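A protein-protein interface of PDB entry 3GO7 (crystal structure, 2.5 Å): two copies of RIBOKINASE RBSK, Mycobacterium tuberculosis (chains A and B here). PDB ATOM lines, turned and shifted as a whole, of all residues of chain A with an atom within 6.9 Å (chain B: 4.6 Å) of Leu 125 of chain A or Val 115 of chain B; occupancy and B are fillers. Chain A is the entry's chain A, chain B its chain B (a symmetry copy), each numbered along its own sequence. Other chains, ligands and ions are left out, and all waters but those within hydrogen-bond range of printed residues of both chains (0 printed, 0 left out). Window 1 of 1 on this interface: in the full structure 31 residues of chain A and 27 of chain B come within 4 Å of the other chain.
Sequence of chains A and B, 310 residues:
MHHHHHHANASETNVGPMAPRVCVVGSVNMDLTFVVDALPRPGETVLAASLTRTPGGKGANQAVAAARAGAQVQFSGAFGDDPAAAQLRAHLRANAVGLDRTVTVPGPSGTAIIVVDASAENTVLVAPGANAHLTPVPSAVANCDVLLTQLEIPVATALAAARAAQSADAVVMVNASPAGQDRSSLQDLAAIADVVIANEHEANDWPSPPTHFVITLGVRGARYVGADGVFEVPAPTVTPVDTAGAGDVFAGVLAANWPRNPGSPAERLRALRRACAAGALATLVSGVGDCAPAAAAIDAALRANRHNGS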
ATOM      1  N   ASN A  29     -24.484  -2.158  29.323  1.00  0.00           N
ATOM      2  CA  ASN A  29     -23.652  -3.371  29.518  1.00  0.00           C
ATOM      3  C   ASN A  29     -23.397  -3.598  30.997  1.00  0.00           C
ATOM      4  O   ASN A  29     -23.404  -2.646  31.793  1.00  0.00           O
ATOM      5  CB  ASN A  29     -22.270  -3.196  28.900  1.00  0.00           C
ATOM      6  CG  ASN A  29     -22.294  -2.902  27.398  1.00  0.00           C
ATOM      7  OD1 ASN A  29     -23.064  -3.495  26.638  1.00  0.00           O
ATOM      8  ND2 ASN A  29     -21.400  -2.008  26.962  1.00  0.00           N
ATOM      9  N   GLY A  43      -0.799 -12.808  24.198  1.00  0.00           N
ATOM     10  CA  GLY A  43      -0.070 -13.976  24.601  1.00  0.00           C
ATOM     11  C   GLY A  43       0.091 -14.091  26.094  1.00  0.00           C
ATOM     12  O   GLY A  43       0.141 -15.201  26.628  1.00  0.00           O
ATOM     13  N   THR A 111     -21.860  -7.268  27.675  1.00  0.00           N
ATOM     14  CA  THR A 111     -20.805  -7.411  28.653  1.00  0.00           C
ATOM     15  C   THR A 111     -19.626  -6.579  28.213  1.00  0.00           C
ATOM     16  O   THR A 111     -19.338  -6.543  27.026  1.00  0.00           O
ATOM     17  CB  THR A 111     -20.348  -8.863  28.764  1.00  0.00           C
ATOM     18  OG1 THR A 111     -21.486  -9.702  28.952  1.00  0.00           O
ATOM     19  CG2 THR A 111     -19.379  -9.047  29.943  1.00  0.00           C
ATOM     20  N   ALA A 112     -18.942  -5.928  29.160  1.00  0.00           N
ATOM     21  CA  ALA A 112     -17.722  -5.209  28.877  1.00  0.00           C
ATOM     22  C   ALA A 112     -16.632  -5.566  29.864  1.00  0.00           C
ATOM     23  O   ALA A 112     -16.889  -5.760  31.069  1.00  0.00           O
ATOM     24  CB  ALA A 112     -17.942  -3.711  28.890  1.00  0.00           C
ATOM     25  N   ILE A 113     -15.405  -5.613  29.352  1.00  0.00           N
ATOM     26  CA  ILE A 113     -14.255  -5.792  30.175  1.00  0.00           C
ATOM     27  C   ILE A 113     -13.509  -4.491  30.108  1.00  0.00           C
ATOM     28  O   ILE A 113     -13.083  -4.063  29.027  1.00  0.00           O
ATOM     29  CB  ILE A 113     -13.354  -6.959  29.643  1.00  0.00           C
ATOM     30  CG1 ILE A 113     -14.192  -8.219  29.347  1.00  0.00           C
ATOM     31  CG2 ILE A 113     -12.226  -7.232  30.577  1.00  0.00           C
ATOM     32  CD1 ILE A 113     -15.043  -8.687  30.477  1.00  0.00           C
ATOM     33  N   ILE A 114     -13.389  -3.842  31.262  1.00  0.00           N
ATOM     34  CA  ILE A 114     -12.514  -2.706  31.414  1.00  0.00           C
ATOM     35  C   ILE A 114     -11.257  -3.135  32.178  1.00  0.00           C
ATOM     36  O   ILE A 114     -11.327  -3.826  33.212  1.00  0.00           O
ATOM     37  CB  ILE A 114     -13.188  -1.525  32.147  1.00  0.00           C
ATOM     38  CG1 ILE A 114     -14.495  -1.132  31.476  1.00  0.00           C
ATOM     39  CG2 ILE A 114     -12.310  -0.295  32.046  1.00  0.00           C
ATOM     40  CD1 ILE A 114     -15.626  -1.897  31.916  1.00  0.00           C
ATOM     41  N   VAL A 115     -10.107  -2.732  31.662  1.00  0.00           N
ATOM     42  CA  VAL A 115      -8.859  -3.005  32.326  1.00  0.00           C
ATOM     43  C   VAL A 115      -8.200  -1.656  32.623  1.00  0.00           C
ATOM     44  O   VAL A 115      -8.017  -0.812  31.720  1.00  0.00           O
ATOM     45  CB  VAL A 115      -7.957  -3.914  31.464  1.00  0.00           C
ATOM     46  CG1 VAL A 115      -6.692  -4.286  32.212  1.00  0.00           C
ATOM     47  CG2 VAL A 115      -8.725  -5.172  31.052  1.00  0.00           C
ATOM     48  N   THR A 123      -8.388   0.063  28.895  1.00  0.00           N
ATOM     49  CA  THR A 123      -8.810  -0.559  27.656  1.00  0.00           C
ATOM     50  C   THR A 123     -10.234  -1.047  27.866  1.00  0.00           C
ATOM     51  O   THR A 123     -10.580  -1.512  28.951  1.00  0.00           O
ATOM     52  CB  THR A 123      -7.951  -1.815  27.299  1.00  0.00           C
ATOM     53  OG1 THR A 123      -8.137  -2.831  28.300  1.00  0.00           O
ATOM     54  CG2 THR A 123      -6.445  -1.492  27.179  1.00  0.00           C
ATOM     55  N   VAL A 124     -11.043  -1.016  26.818  1.00  0.00           N
ATOM     56  CA  VAL A 124     -12.430  -1.445  26.925  1.00  0.00           C
ATOM     57  C   VAL A 124     -12.720  -2.458  25.828  1.00  0.00           C
ATOM     58  O   VAL A 124     -12.449  -2.212  24.653  1.00  0.00           O
ATOM     59  CB  VAL A 124     -13.434  -0.224  26.816  1.00  0.00           C
ATOM     60  CG1 VAL A 124     -14.875  -0.694  26.679  1.00  0.00           C
ATOM     61  CG2 VAL A 124     -13.277   0.747  27.984  1.00  0.00           C
ATOM     62  N   LEU A 125     -13.296  -3.584  26.215  1.00  0.00           N
ATOM     63  CA  LEU A 125     -13.692  -4.612  25.295  1.00  0.00           C
ATOM     64  C   LEU A 125     -15.159  -5.020  25.550  1.00  0.00           C
ATOM     65  O   LEU A 125     -15.517  -5.352  26.669  1.00  0.00           O
ATOM     66  CB  LEU A 125     -12.774  -5.804  25.507  1.00  0.00           C
ATOM     67  CG  LEU A 125     -13.170  -7.068  24.751  1.00  0.00           C
ATOM     68  CD1 LEU A 125     -12.903  -6.843  23.283  1.00  0.00           C
ATOM     69  CD2 LEU A 125     -12.414  -8.286  25.292  1.00  0.00           C
ATOM     70  N   VAL A 126     -15.988  -5.031  24.507  1.00  0.00           N
ATOM     71  CA  VAL A 126     -17.419  -5.191  24.671  1.00  0.00           C
ATOM     72  C   VAL A 126     -17.970  -6.361  23.860  1.00  0.00           C
ATOM     73  O   VAL A 126     -17.661  -6.477  22.679  1.00  0.00           O
ATOM     74  CB  VAL A 126     -18.159  -3.912  24.210  1.00  0.00           C
ATOM     75  CG1 VAL A 126     -19.640  -4.067  24.381  1.00  0.00           C
ATOM     76  CG2 VAL A 126     -17.656  -2.686  24.954  1.00  0.00           C
ATOM     77  N   ALA A 127     -18.761  -7.228  24.485  1.00  0.00           N
ATOM     78  CA  ALA A 127     -19.591  -8.145  23.736  1.00  0.00           C
ATOM     79  C   ALA A 127     -20.981  -7.537  23.857  1.00  0.00           C
ATOM     80  O   ALA A 127     -21.582  -7.589  24.929  1.00  0.00           O
ATOM     81  CB  ALA A 127     -19.550  -9.529  24.295  1.00  0.00           C
ATOM     82  N   PHE B  34     -13.615 -14.256  24.620  1.00  0.00           N
ATOM     83  CA  PHE B  34     -13.949 -13.217  23.640  1.00  0.00           C
ATOM     84  C   PHE B  34     -13.149 -13.451  22.349  1.00  0.00           C
ATOM     85  O   PHE B  34     -11.918 -13.526  22.395  1.00  0.00           O
ATOM     86  CB  PHE B  34     -13.570 -11.835  24.185  1.00  0.00           C
ATOM     87  CG  PHE B  34     -14.446 -11.343  25.292  1.00  0.00           C
ATOM     88  CD1 PHE B  34     -15.519 -10.499  25.022  1.00  0.00           C
ATOM     89  CD2 PHE B  34     -14.180 -11.688  26.618  1.00  0.00           C
ATOM     90  CE1 PHE B  34     -16.342 -10.053  26.049  1.00  0.00           C
ATOM     91  CE2 PHE B  34     -15.001 -11.238  27.678  1.00  0.00           C
ATOM     92  CZ  PHE B  34     -16.068 -10.436  27.408  1.00  0.00           C
ATOM     93  N   VAL B  36     -11.884 -11.663  19.131  1.00  0.00           N
ATOM     94  CA  VAL B  36     -11.667 -10.292  18.653  1.00  0.00           C
ATOM     95  C   VAL B  36     -10.711 -10.282  17.466  1.00  0.00           C
ATOM     96  O   VAL B  36      -9.954 -11.222  17.243  1.00  0.00           O
ATOM     97  CB  VAL B  36     -11.027  -9.363  19.742  1.00  0.00           C
ATOM     98  CG1 VAL B  36     -11.891  -9.318  20.990  1.00  0.00           C
ATOM     99  CG2 VAL B  36      -9.573  -9.795  20.094  1.00  0.00           C
ATOM    100  N   LEU B  39      -6.695  -7.170  20.295  1.00  0.00           N
ATOM    101  CA  LEU B  39      -6.810  -6.594  21.627  1.00  0.00           C
ATOM    102  C   LEU B  39      -7.000  -5.094  21.544  1.00  0.00           C
ATOM    103  O   LEU B  39      -6.446  -4.460  20.661  1.00  0.00           O
ATOM    104  CB  LEU B  39      -5.551  -6.851  22.461  1.00  0.00           C
ATOM    105  CG  LEU B  39      -5.313  -8.222  23.109  1.00  0.00           C
ATOM    106  CD1 LEU B  39      -4.130  -8.138  24.083  1.00  0.00           C
ATOM    107  CD2 LEU B  39      -6.567  -8.761  23.836  1.00  0.00           C
ATOM    108  N   PRO B  40      -7.776  -4.516  22.475  1.00  0.00           N
ATOM    109  CA  PRO B  40      -7.940  -3.078  22.476  1.00  0.00           C
ATOM    110  C   PRO B  40      -6.664  -2.336  22.888  1.00  0.00           C
ATOM    111  O   PRO B  40      -6.008  -2.702  23.860  1.00  0.00           O
ATOM    112  CB  PRO B  40      -9.024  -2.859  23.525  1.00  0.00           C
ATOM    113  CG  PRO B  40      -8.888  -4.024  24.439  1.00  0.00           C
ATOM    114  CD  PRO B  40      -8.526  -5.165  23.565  1.00  0.00           C
ATOM    115  N   VAL B  46     -13.144  -1.754  21.745  1.00  0.00           N
ATOM    116  CA  VAL B  46     -13.194  -2.748  20.695  1.00  0.00           C
ATOM    117  C   VAL B  46     -14.428  -3.611  20.912  1.00  0.00           C
ATOM    118  O   VAL B  46     -14.792  -3.879  22.062  1.00  0.00           O
ATOM    119  CB  VAL B  46     -11.882  -3.626  20.710  1.00  0.00           C
ATOM    120  CG1 VAL B  46     -12.113  -4.952  20.051  1.00  0.00           C
ATOM    121  CG2 VAL B  46     -10.712  -2.872  20.040  1.00  0.00           C
ATOM    122  N   ALA B  48     -16.254  -7.338  20.387  1.00  0.00           N
ATOM    123  CA  ALA B  48     -15.958  -8.732  20.148  1.00  0.00           C
ATOM    124  C   ALA B  48     -16.953  -9.262  19.114  1.00  0.00           C
ATOM    125  O   ALA B  48     -18.092  -8.782  19.032  1.00  0.00           O
ATOM    126  CB  ALA B  48     -16.034  -9.522  21.440  1.00  0.00           C
ATOM    127  N   ILE B 113     -10.736 -14.030  31.915  1.00  0.00           N
ATOM    128  CA  ILE B 113     -11.029 -13.428  30.619  1.00  0.00           C
ATOM    129  C   ILE B 113     -10.021 -13.964  29.625  1.00  0.00           C
ATOM    130  O   ILE B 113      -8.824 -13.777  29.827  1.00  0.00           O
ATOM    131  CB  ILE B 113     -10.899 -11.872  30.625  1.00  0.00           C
ATOM    132  CG1 ILE B 113     -11.769 -11.219  31.717  1.00  0.00           C
ATOM    133  CG2 ILE B 113     -11.200 -11.295  29.235  1.00  0.00           C
ATOM    134  CD1 ILE B 113     -13.250 -11.681  31.791  1.00  0.00           C
ATOM    135  N   ILE B 114     -10.509 -14.619  28.559  1.00  0.00           N
ATOM    136  CA  ILE B 114      -9.670 -15.199  27.517  1.00  0.00           C
ATOM    137  C   ILE B 114      -9.966 -14.549  26.163  1.00  0.00           C
ATOM    138  O   ILE B 114     -11.041 -14.742  25.581  1.00  0.00           O
ATOM    139  CB  ILE B 114      -9.854 -16.726  27.426  1.00  0.00           C
ATOM    140  CG1 ILE B 114      -9.608 -17.392  28.788  1.00  0.00           C
ATOM    141  CG2 ILE B 114      -8.919 -17.323  26.360  1.00  0.00           C
ATOM    142  CD1 ILE B 114     -10.856 -17.785  29.540  1.00  0.00           C
ATOM    143  N   VAL B 115      -9.011 -13.784  25.660  1.00  0.00           N
ATOM    144  CA  VAL B 115      -9.170 -13.157  24.365  1.00  0.00           C
ATOM    145  C   VAL B 115      -8.361 -13.832  23.261  1.00  0.00           C
ATOM    146  O   VAL B 115      -7.135 -13.878  23.312  1.00  0.00           O
ATOM    147  CB  VAL B 115      -8.800 -11.678  24.405  1.00  0.00           C
ATOM    148  CG1 VAL B 115      -9.121 -11.067  23.066  1.00  0.00           C
ATOM    149  CG2 VAL B 115      -9.559 -10.952  25.526  1.00  0.00           C
ATOM    150  N   VAL B 116      -9.076 -14.356  22.273  1.00  0.00           N
ATOM    151  CA  VAL B 116      -8.514 -14.966  21.074  1.00  0.00           C
ATOM    152  C   VAL B 116      -8.544 -13.929  19.976  1.00  0.00           C
ATOM    153  O   VAL B 116      -9.612 -13.425  19.630  1.00  0.00           O
ATOM    154  CB  VAL B 116      -9.385 -16.161  20.618  1.00  0.00           C
ATOM    155  CG1 VAL B 116      -8.656 -17.000  19.548  1.00  0.00           C
ATOM    156  CG2 VAL B 116      -9.770 -17.030  21.807  1.00  0.00           C
ATOM    157  N   ASP B 117      -7.384 -13.586  19.422  1.00  0.00           N
ATOM    158  CA  ASP B 117      -7.374 -12.624  18.318  1.00  0.00           C
ATOM    159  C   ASP B 117      -7.168 -13.291  17.007  1.00  0.00           C
ATOM    160  O   ASP B 117      -7.066 -14.509  16.931  1.00  0.00           O
ATOM    161  CB  ASP B 117      -6.375 -11.474  18.500  1.00  0.00           C
ATOM    162  CG  ASP B 117      -4.961 -11.945  18.671  1.00  0.00           C
ATOM    163  OD1 ASP B 117      -4.541 -12.903  17.981  1.00  0.00           O
ATOM    164  OD2 ASP B 117      -4.265 -11.337  19.508  1.00  0.00           O
ATOM    165  N   GLU B 121      -3.462 -15.728  18.834  1.00  0.00           N
ATOM    166  CA  GLU B 121      -2.838 -15.546  20.154  1.00  0.00           C
ATOM    167  C   GLU B 121      -3.921 -15.512  21.248  1.00  0.00           C
ATOM    168  O   GLU B 121      -5.013 -14.974  21.010  1.00  0.00           O
ATOM    169  CB  GLU B 121      -2.065 -14.216  20.181  1.00  0.00           C
ATOM    170  CG  GLU B 121      -0.697 -14.236  19.526  1.00  0.00           C
ATOM    171  CD  GLU B 121       0.380 -14.697  20.497  1.00  0.00           C
ATOM    172  OE1 GLU B 121       0.247 -15.807  21.086  1.00  0.00           O
ATOM    173  OE2 GLU B 121       1.352 -13.935  20.683  1.00  0.00           O
ATOM    174  N   ASN B 122      -3.622 -16.073  22.424  1.00  0.00           N
ATOM    175  CA  ASN B 122      -4.531 -16.029  23.583  1.00  0.00           C
ATOM    176  C   ASN B 122      -4.011 -15.143  24.686  1.00  0.00           C
ATOM    177  O   ASN B 122      -2.924 -15.386  25.194  1.00  0.00           O
ATOM    178  CB  ASN B 122      -4.752 -17.411  24.186  1.00  0.00           C
ATOM    179  CG  ASN B 122      -5.774 -18.220  23.433  1.00  0.00           C
ATOM    180  OD1 ASN B 122      -5.859 -18.157  22.199  1.00  0.00           O
ATOM    181  ND2 ASN B 122      -6.563 -18.997  24.173  1.00  0.00           N
ATOM    182  N   THR B 123      -4.795 -14.136  25.070  1.00  0.00           N
ATOM    183  CA  THR B 123      -4.463 -13.296  26.211  1.00  0.00           C
ATOM    184  C   THR B 123      -5.403 -13.599  27.365  1.00  0.00           C
ATOM    185  O   THR B 123      -6.618 -13.592  27.195  1.00  0.00           O
ATOM    186  CB  THR B 123      -4.584 -11.844  25.856  1.00  0.00           C
ATOM    187  OG1 THR B 123      -3.917 -11.628  24.611  1.00  0.00           O
ATOM    188  CG2 THR B 123      -3.929 -10.999  26.922  1.00  0.00           C
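The backbone NH (N) of Val 36 of chain B sits at hydrogen-bond distance from the backbone carbonyl oxygen (O) of Val 116 of chain B (2.9 Å).
The backbone NH of Glu 121 of chain B sits at hydrogen-bond distance from the side-chain carboxylate of Asp 117 of chain B (3.1 Å).
O of Ile 114 of chain B lies within hydrogen-bond range of N of Phe 34 of chain B (2.8 Å).
The backbone carbonyl oxygen (O) of Leu 125 of chain A sits at hydrogen-bond distance from the backbone NH (N) of Ile 113 of chain A (2.7 Å).
N of Ala 127 of chain A is in hydrogen-bond range of O of Thr 111 of chain A (2.7 Å).
O of Phe 34 of chain B lies within hydrogen-bond range of N of Val 116 of chain B (3.0 Å).
Ile 113 of chain B touches its own counterpart, Ile 113 of chain A.
The backbone NH of Val 46 of chain B is in hydrogen-bond range of the backbone carbonyl oxygen of Val 124 of chain A (3.0 Å).
The backbone NH (N) of Val 126 of chain A is in hydrogen-bond range of the backbone carbonyl oxygen (O) of Val 46 of chain B (3.0 Å).
The backbone NH (N) of Gly 43 of chain A is in hydrogen-bond range of the side-chain hydroxyl (OG1) of Thr 123 of chain B (3.4 Å).
The backbone carbonyl oxygen (O) of Val 126 of chain A sits at hydrogen-bond distance from the backbone NH (N) of Ala 48 of chain B, at 2.8 Å.
The backbone NH (N) of Gly 43 of chain A sits close to the backbone carbonyl oxygen (O) of Asn 122 of chain B (3.5 Å).
Ala 112 of chain A touches none of the printed residues of chain B.
Leu 125 of chain A touches just these residues of chain B: Phe 34, Val 36, Val 46 and Val 115.
Printed residues of chain B within 4 Å of Val 126 of chain A: Val 46 (3.0 Å) and Ala 48 (2.8 Å).
Of the printed residues of chain A, Val 115 of chain B touches Leu 125 (3.9 Å).
Of the printed residues of chain A, Glu 121 of chain B touches Gly 43.
Printed residues of chain A within 4 Å of Thr 123 of chain B: Gly 43.
The nearest residue of chain B that does not touch Leu 125 of chain A is Pro 40 of chain B (4.4 Å).
The nearest printed residue of chain A that does not touch Val 46 of chain B is Ala 127 of chain A (5.7 Å).
Hydrophobic or aromatic side chains of chain A that line the printed part of chain B: Ile 113, Leu 125, Val 126 and Ala 127.
Of the 14 printed residues of chain B, 10 touch a printed residue of chain A.
Hydrophobic or aromatic side chains of chain B within 4 Å of the printed part of chain A: Phe 34, Val 36, Pro 40, Val 46, Ala 48, Ile 113 and Val 115.
Among the printed residues, no Asp or Glu carboxylate lies within 4 Å of a Lys or Arg side-chain nitrogen of the other chain.
Among the printed residues, pairs that only touch across the chains: Gly 43 of chain A with Glu 121 of chain B (3.98 Å), Ile 113 of chain A with Phe 34 of chain B (3.5 Å), Ile 113 of chain A with Ile 113 of chain B (3.7 Å), Thr 123 of chain A with Pro 40 of chain B (3.6 Å), Val 124 of chain A with Pro 40 of chain B (3.7 Å), Leu 125 of chain A with Phe 34 of chain B (3.7 Å), Leu 125 of chain A with Val 36 of chain B (3.5 Å), Leu 125 of chain A with Val 46 of chain B (3.5 Å), Leu 125 of chain A with Val 115 of chain B (3.9 Å) and Ala 127 of chain A with Phe 34 of chain B (3.7 Å).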
